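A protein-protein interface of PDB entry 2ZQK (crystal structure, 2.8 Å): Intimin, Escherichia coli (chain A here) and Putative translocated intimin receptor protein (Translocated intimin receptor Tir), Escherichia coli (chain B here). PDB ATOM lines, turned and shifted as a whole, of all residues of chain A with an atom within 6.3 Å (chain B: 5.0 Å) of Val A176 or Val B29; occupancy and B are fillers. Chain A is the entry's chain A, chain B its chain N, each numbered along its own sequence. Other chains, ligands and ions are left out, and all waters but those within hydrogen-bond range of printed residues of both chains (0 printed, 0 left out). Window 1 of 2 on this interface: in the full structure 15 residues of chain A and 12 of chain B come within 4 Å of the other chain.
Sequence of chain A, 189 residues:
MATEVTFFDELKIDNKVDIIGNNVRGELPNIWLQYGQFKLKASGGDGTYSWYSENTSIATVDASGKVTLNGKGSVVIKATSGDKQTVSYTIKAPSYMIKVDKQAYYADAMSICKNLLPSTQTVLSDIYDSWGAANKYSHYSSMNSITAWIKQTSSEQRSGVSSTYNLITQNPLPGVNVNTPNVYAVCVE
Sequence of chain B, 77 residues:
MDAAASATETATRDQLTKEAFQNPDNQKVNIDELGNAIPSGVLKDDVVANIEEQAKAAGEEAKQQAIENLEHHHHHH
O of Gly A160 is in hydrogen-bond range of NZ of Lys B28, 2.7 Å away.
The backbone NH (N) of Asn A177 sits at hydrogen-bond distance from the backbone carbonyl oxygen (O) of Val B29, at 2.8 Å.
The side-chain amide nitrogen of Asn A177 is in hydrogen-bond range of the side-chain amide oxygen of Asn B30, 3.3 Å away.
The backbone NH (N) of Ile B31 sits at hydrogen-bond distance from the side-chain hydroxyl (OG1) of Thr A180 (2.8 Å).
OG1 of Thr A180 lies close to OD1 of Asn B30, 3.5 Å away.
O of Gly A175 is in hydrogen-bond range of N of Val B29 (3.0 Å).
O of Val A176 lies within hydrogen-bond range of N of Ser A162 (3.0 Å).
The backbone carbonyl oxygen of Ile B38 lies within hydrogen-bond range of the backbone NH of Asn B30.
N of Val A178 lies close to O of Gly A160.
The backbone carbonyl oxygen (O) of Lys B28 lies within hydrogen-bond range of the side-chain hydroxyl (OG) of Ser B40, 2.6 Å away.
OD1 of Asn A177 sits at hydrogen-bond distance from N of Asn A179, at 2.6 Å.
The side-chain hydroxyl of Thr A164 sits at hydrogen-bond distance from the backbone carbonyl oxygen of Leu A173.
Val A161 touches Lys B28.
CD1 of Ile B31 touches CD1 of Leu A173 (3.7 Å).
N of Ala B37 touches CD1 of Leu A173 (3.96 Å).
Gly A175 touches Lys B28 (O to CA, 3.7 Å).
CA of Val A176 touches O of Val B29, at 3.5 Å.
Asn A177 touches Lys B28 (CA to CD, 3.9 Å).
Val A176 touches one residue of chain B.
Val B29 touches just these residues of chain A: Gly A175, Val A176 and Asn A177.
Printed residues of chain A within 4 Å of Lys B28: Gly A160, Val A161, Gly A175 and Asn A177.
Printed residues of chain B within 4 Å of Val A161: Lys B28.
Printed residues of chain B within 4 Å of Leu A173: Ile B31 (3.7 Å) and Ala B37 (3.96 Å).
Of the printed residues of chain B, Gly A160 touches Lys B28.
Of the printed residues of chain B, Gly A175 touches Lys B28 and Val B29.
The nearest residue of chain B that does not touch Val A176 is Ile B31 (4.2 Å).
Printed residues of chain B that touch a printed residue of chain A: Lys B28, Val B29, Asn B30, Ile B31 and Ala B37.
Hydrophobic or aromatic side chains of chain B within 4 Å of the printed part of chain A: Val B29 and Ile B31.
Of the 15 printed residues of chain A, 7 touch a printed residue of chain B.
Printed residues of chain A that touch a printed residue of chain B: Gly A160, Val A161, Leu A173, Gly A175, Val A176, Asn A177 and Thr A180.
Hydrophobic or aromatic side chains of chain A that line the printed part of chain B: Val A161, Leu A173 and Val A176.
Among the printed residues, no Asp or Glu carboxylate lies within 4 Å of a Lys or Arg side-chain nitrogen of the other chain.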
ATOM      1  N   TRP A 149      23.838  32.207 -10.808  1.00  0.00           N
ATOM      2  CA  TRP A 149      23.216  31.461  -9.706  1.00  0.00           C
ATOM      3  C   TRP A 149      21.817  31.934  -9.352  1.00  0.00           C
ATOM      4  O   TRP A 149      21.553  33.124  -9.351  1.00  0.00           O
ATOM      5  CB  TRP A 149      24.058  31.609  -8.446  1.00  0.00           C
ATOM      6  CG  TRP A 149      25.278  30.776  -8.397  1.00  0.00           C
ATOM      7  CD1 TRP A 149      26.578  31.210  -8.259  1.00  0.00           C
ATOM      8  CD2 TRP A 149      25.326  29.349  -8.365  1.00  0.00           C
ATOM      9  NE1 TRP A 149      27.426  30.131  -8.129  1.00  0.00           N
ATOM     10  CE2 TRP A 149      26.684  28.979  -8.193  1.00  0.00           C
ATOM     11  CE3 TRP A 149      24.356  28.349  -8.461  1.00  0.00           C
ATOM     12  CZ2 TRP A 149      27.088  27.645  -8.115  1.00  0.00           C
ATOM     13  CZ3 TRP A 149      24.758  27.028  -8.383  1.00  0.00           C
ATOM     14  CH2 TRP A 149      26.116  26.685  -8.211  1.00  0.00           C
ATOM     15  N   GLY A 160      21.998  19.636  -2.347  1.00  0.00           N
ATOM     16  CA  GLY A 160      23.362  20.049  -2.620  1.00  0.00           C
ATOM     17  C   GLY A 160      23.565  20.710  -3.960  1.00  0.00           C
ATOM     18  O   GLY A 160      24.664  20.667  -4.519  1.00  0.00           O
ATOM     19  N   VAL A 161      22.510  21.338  -4.471  1.00  0.00           N
ATOM     20  CA  VAL A 161      22.577  21.982  -5.771  1.00  0.00           C
ATOM     21  C   VAL A 161      21.674  23.170  -5.718  1.00  0.00           C
ATOM     22  O   VAL A 161      21.021  23.409  -4.704  1.00  0.00           O
ATOM     23  CB  VAL A 161      22.040  21.064  -6.923  1.00  0.00           C
ATOM     24  CG1 VAL A 161      22.778  19.718  -6.931  1.00  0.00           C
ATOM     25  CG2 VAL A 161      20.532  20.855  -6.775  1.00  0.00           C
ATOM     26  N   SER A 162      21.623  23.883  -6.839  1.00  0.00           N
ATOM     27  CA  SER A 162      20.797  25.075  -7.007  1.00  0.00           C
ATOM     28  C   SER A 162      20.535  25.245  -8.521  1.00  0.00           C
ATOM     29  O   SER A 162      21.155  24.565  -9.341  1.00  0.00           O
ATOM     30  CB  SER A 162      21.534  26.287  -6.431  1.00  0.00           C
ATOM     31  OG  SER A 162      20.797  27.472  -6.627  1.00  0.00           O
ATOM     32  N   SER A 163      19.609  26.122  -8.893  1.00  0.00           N
ATOM     33  CA  SER A 163      19.325  26.346 -10.305  1.00  0.00           C
ATOM     34  C   SER A 163      20.253  27.396 -10.891  1.00  0.00           C
ATOM     35  O   SER A 163      21.123  27.908 -10.195  1.00  0.00           O
ATOM     36  CB  SER A 163      17.879  26.769 -10.500  1.00  0.00           C
ATOM     37  OG  SER A 163      17.045  25.632 -10.392  1.00  0.00           O
ATOM     38  N   THR A 164      20.076  27.709 -12.172  1.00  0.00           N
ATOM     39  CA  THR A 164      20.925  28.687 -12.857  1.00  0.00           C
ATOM     40  C   THR A 164      20.219  29.223 -14.091  1.00  0.00           C
ATOM     41  O   THR A 164      19.287  28.604 -14.605  1.00  0.00           O
ATOM     42  CB  THR A 164      22.262  28.058 -13.354  1.00  0.00           C
ATOM     43  OG1 THR A 164      21.956  26.873 -14.095  1.00  0.00           O
ATOM     44  CG2 THR A 164      23.208  27.698 -12.198  1.00  0.00           C
ATOM     45  N   LEU A 173      19.193  26.001 -16.284  1.00  0.00           N
ATOM     46  CA  LEU A 173      19.537  24.637 -15.922  1.00  0.00           C
ATOM     47  C   LEU A 173      19.355  24.394 -14.435  1.00  0.00           C
ATOM     48  O   LEU A 173      19.841  25.149 -13.600  1.00  0.00           O
ATOM     49  CB  LEU A 173      20.982  24.335 -16.293  1.00  0.00           C
ATOM     50  CG  LEU A 173      21.204  24.258 -17.791  1.00  0.00           C
ATOM     51  CD1 LEU A 173      22.676  24.088 -18.101  1.00  0.00           C
ATOM     52  CD2 LEU A 173      20.417  23.073 -18.323  1.00  0.00           C
ATOM     53  N   PRO A 174      18.608  23.353 -14.090  1.00  0.00           N
ATOM     54  CA  PRO A 174      18.354  22.978 -12.700  1.00  0.00           C
ATOM     55  C   PRO A 174      19.400  21.910 -12.341  1.00  0.00           C
ATOM     56  O   PRO A 174      20.243  21.573 -13.166  1.00  0.00           O
ATOM     57  CB  PRO A 174      16.960  22.398 -12.770  1.00  0.00           C
ATOM     58  CG  PRO A 174      17.030  21.647 -14.087  1.00  0.00           C
ATOM     59  CD  PRO A 174      17.652  22.689 -14.996  1.00  0.00           C
ATOM     60  N   GLY A 175      19.340  21.377 -11.123  1.00  0.00           N
ATOM     61  CA  GLY A 175      20.279  20.348 -10.687  1.00  0.00           C
ATOM     62  C   GLY A 175      21.766  20.665 -10.750  1.00  0.00           C
ATOM     63  O   GLY A 175      22.598  19.749 -10.852  1.00  0.00           O
ATOM     64  N   VAL A 176      22.127  21.940 -10.656  1.00  0.00           N
ATOM     65  CA  VAL A 176      23.542  22.294 -10.749  1.00  0.00           C
ATOM     66  C   VAL A 176      24.331  22.210  -9.454  1.00  0.00           C
ATOM     67  O   VAL A 176      23.959  22.795  -8.441  1.00  0.00           O
ATOM     68  CB  VAL A 176      23.735  23.716 -11.354  1.00  0.00           C
ATOM     69  CG1 VAL A 176      25.214  24.034 -11.471  1.00  0.00           C
ATOM     70  CG2 VAL A 176      23.073  23.801 -12.731  1.00  0.00           C
ATOM     71  N   ASN A 177      25.432  21.466  -9.522  1.00  0.00           N
ATOM     72  CA  ASN A 177      26.365  21.253  -8.411  1.00  0.00           C
ATOM     73  C   ASN A 177      26.688  22.622  -7.861  1.00  0.00           C
ATOM     74  O   ASN A 177      27.038  23.521  -8.610  1.00  0.00           O
ATOM     75  CB  ASN A 177      27.650  20.615  -8.950  1.00  0.00           C
ATOM     76  CG  ASN A 177      28.679  20.300  -7.864  1.00  0.00           C
ATOM     77  OD1 ASN A 177      28.655  20.869  -6.779  1.00  0.00           O
ATOM     78  ND2 ASN A 177      29.606  19.392  -8.177  1.00  0.00           N
ATOM     79  N   VAL A 178      26.554  22.790  -6.556  1.00  0.00           N
ATOM     80  CA  VAL A 178      26.869  24.061  -5.925  1.00  0.00           C
ATOM     81  C   VAL A 178      28.339  24.399  -6.145  1.00  0.00           C
ATOM     82  O   VAL A 178      28.694  25.557  -6.236  1.00  0.00           O
ATOM     83  CB  VAL A 178      26.601  23.992  -4.421  1.00  0.00           C
ATOM     84  CG1 VAL A 178      25.113  24.112  -4.148  1.00  0.00           C
ATOM     85  CG2 VAL A 178      27.117  22.692  -3.876  1.00  0.00           C
ATOM     86  N   ASN A 179      29.184  23.379  -6.246  1.00  0.00           N
ATOM     87  CA  ASN A 179      30.615  23.563  -6.443  1.00  0.00           C
ATOM     88  C   ASN A 179      31.115  23.489  -7.865  1.00  0.00           C
ATOM     89  O   ASN A 179      32.211  22.966  -8.110  1.00  0.00           O
ATOM     90  CB  ASN A 179      31.407  22.532  -5.661  1.00  0.00           C
ATOM     91  CG  ASN A 179      31.354  22.765  -4.199  1.00  0.00           C
ATOM     92  OD1 ASN A 179      31.337  23.909  -3.734  1.00  0.00           O
ATOM     93  ND2 ASN A 179      31.345  21.684  -3.444  1.00  0.00           N
ATOM     94  N   THR A 180      30.347  23.991  -8.814  1.00  0.00           N
ATOM     95  CA  THR A 180      30.837  23.927 -10.170  1.00  0.00           C
ATOM     96  C   THR A 180      31.520  25.234 -10.488  1.00  0.00           C
ATOM     97  O   THR A 180      31.171  26.283  -9.947  1.00  0.00           O
ATOM     98  CB  THR A 180      29.711  23.731 -11.204  1.00  0.00           C
ATOM     99  OG1 THR A 180      30.288  23.615 -12.508  1.00  0.00           O
ATOM    100  CG2 THR A 180      28.775  24.926 -11.204  1.00  0.00           C
ATOM    101  N   VAL A 183      30.311  29.607 -12.938  1.00  0.00           N
ATOM    102  CA  VAL A 183      29.001  30.164 -12.606  1.00  0.00           C
ATOM    103  C   VAL A 183      29.292  31.468 -11.890  1.00  0.00           C
ATOM    104  O   VAL A 183      30.010  31.475 -10.902  1.00  0.00           O
ATOM    105  CB  VAL A 183      28.186  29.233 -11.709  1.00  0.00           C
ATOM    106  CG1 VAL A 183      26.754  29.680 -11.681  1.00  0.00           C
ATOM    107  CG2 VAL A 183      28.227  27.832 -12.252  1.00  0.00           C
ATOM    108  N   GLN B  27      22.026  12.488 -10.169  1.00  0.00           N
ATOM    109  CA  GLN B  27      23.331  13.099 -10.353  1.00  0.00           C
ATOM    110  C   GLN B  27      23.354  14.618 -10.550  1.00  0.00           C
ATOM    111  O   GLN B  27      22.514  15.189 -11.250  1.00  0.00           O
ATOM    112  CB  GLN B  27      24.034  12.433 -11.525  1.00  0.00           C
ATOM    113  CG  GLN B  27      25.543  12.527 -11.467  1.00  0.00           C
ATOM    114  CD  GLN B  27      26.195  11.977 -12.716  1.00  0.00           C
ATOM    115  OE1 GLN B  27      25.722  10.994 -13.293  1.00  0.00           O
ATOM    116  NE2 GLN B  27      27.294  12.601 -13.135  1.00  0.00           N
ATOM    117  N   LYS B  28      24.337  15.259  -9.918  1.00  0.00           N
ATOM    118  CA  LYS B  28      24.534  16.699 -10.011  1.00  0.00           C
ATOM    119  C   LYS B  28      25.190  17.005 -11.342  1.00  0.00           C
ATOM    120  O   LYS B  28      25.827  16.145 -11.936  1.00  0.00           O
ATOM    121  CB  LYS B  28      25.454  17.192  -8.897  1.00  0.00           C
ATOM    122  CG  LYS B  28      24.896  17.062  -7.489  1.00  0.00           C
ATOM    123  CD  LYS B  28      25.773  17.845  -6.529  1.00  0.00           C
ATOM    124  CE  LYS B  28      25.405  17.611  -5.084  1.00  0.00           C
ATOM    125  NZ  LYS B  28      26.189  18.511  -4.215  1.00  0.00           N
ATOM    126  N   VAL B  29      25.051  18.238 -11.802  1.00  0.00           N
ATOM    127  CA  VAL B  29      25.638  18.652 -13.068  1.00  0.00           C
ATOM    128  C   VAL B  29      26.589  19.851 -12.906  1.00  0.00           C
ATOM    129  O   VAL B  29      26.368  20.736 -12.071  1.00  0.00           O
ATOM    130  CB  VAL B  29      24.507  19.001 -14.062  1.00  0.00           C
ATOM    131  CG1 VAL B  29      24.944  20.084 -15.012  1.00  0.00           C
ATOM    132  CG2 VAL B  29      24.104  17.755 -14.835  1.00  0.00           C
ATOM    133  N   ASN B  30      27.655  19.876 -13.696  1.00  0.00           N
ATOM    134  CA  ASN B  30      28.597  20.991 -13.645  1.00  0.00           C
ATOM    135  C   ASN B  30      28.309  21.906 -14.829  1.00  0.00           C
ATOM    136  O   ASN B  30      27.354  21.680 -15.562  1.00  0.00           O
ATOM    137  CB  ASN B  30      30.049  20.499 -13.702  1.00  0.00           C
ATOM    138  CG  ASN B  30      30.559  20.008 -12.348  1.00  0.00           C
ATOM    139  OD1 ASN B  30      30.008  20.365 -11.296  1.00  0.00           O
ATOM    140  ND2 ASN B  30      31.626  19.205 -12.366  1.00  0.00           N
ATOM    141  N   ILE B  31      29.124  22.939 -15.010  1.00  0.00           N
ATOM    142  CA  ILE B  31      28.941  23.868 -16.110  1.00  0.00           C
ATOM    143  C   ILE B  31      30.268  24.253 -16.745  1.00  0.00           C
ATOM    144  O   ILE B  31      31.172  24.739 -16.063  1.00  0.00           O
ATOM    145  CB  ILE B  31      28.221  25.112 -15.642  1.00  0.00           C
ATOM    146  CG1 ILE B  31      26.772  24.755 -15.268  1.00  0.00           C
ATOM    147  CG2 ILE B  31      28.314  26.200 -16.711  1.00  0.00           C
ATOM    148  CD1 ILE B  31      25.956  24.172 -16.395  1.00  0.00           C
ATOM    149  N   ALA B  37      25.826  22.191 -19.574  1.00  0.00           N
ATOM    150  CA  ALA B  37      25.846  21.152 -18.575  1.00  0.00           C
ATOM    151  C   ALA B  37      26.849  20.083 -18.883  1.00  0.00           C
ATOM    152  O   ALA B  37      27.200  19.888 -20.030  1.00  0.00           O
ATOM    153  CB  ALA B  37      24.501  20.538 -18.502  1.00  0.00           C
ATOM    154  N   ILE B  38      27.326  19.394 -17.854  1.00  0.00           N
ATOM    155  CA  ILE B  38      28.230  18.261 -18.048  1.00  0.00           C
ATOM    156  C   ILE B  38      28.203  17.382 -16.816  1.00  0.00           C
ATOM    157  O   ILE B  38      27.969  17.858 -15.707  1.00  0.00           O
ATOM    158  CB  ILE B  38      29.728  18.635 -18.310  1.00  0.00           C
ATOM    159  CG1 ILE B  38      30.222  19.674 -17.303  1.00  0.00           C
ATOM    160  CG2 ILE B  38      29.908  19.065 -19.731  1.00  0.00           C
ATOM    161  CD1 ILE B  38      31.728  19.639 -17.103  1.00  0.00           C
ATOM    162  N   SER B  40      29.041  15.590 -13.512  1.00  0.00           N
ATOM    163  CA  SER B  40      29.853  16.098 -12.413  1.00  0.00           C
ATOM    164  C   SER B  40      30.556  14.970 -11.673  1.00  0.00           C
ATOM    165  O   SER B  40      31.622  15.166 -11.086  1.00  0.00           O
ATOM    166  CB  SER B  40      28.967  16.840 -11.435  1.00  0.00           C
ATOM    167  OG  SER B  40      28.153  15.908 -10.746  1.00  0.00           O
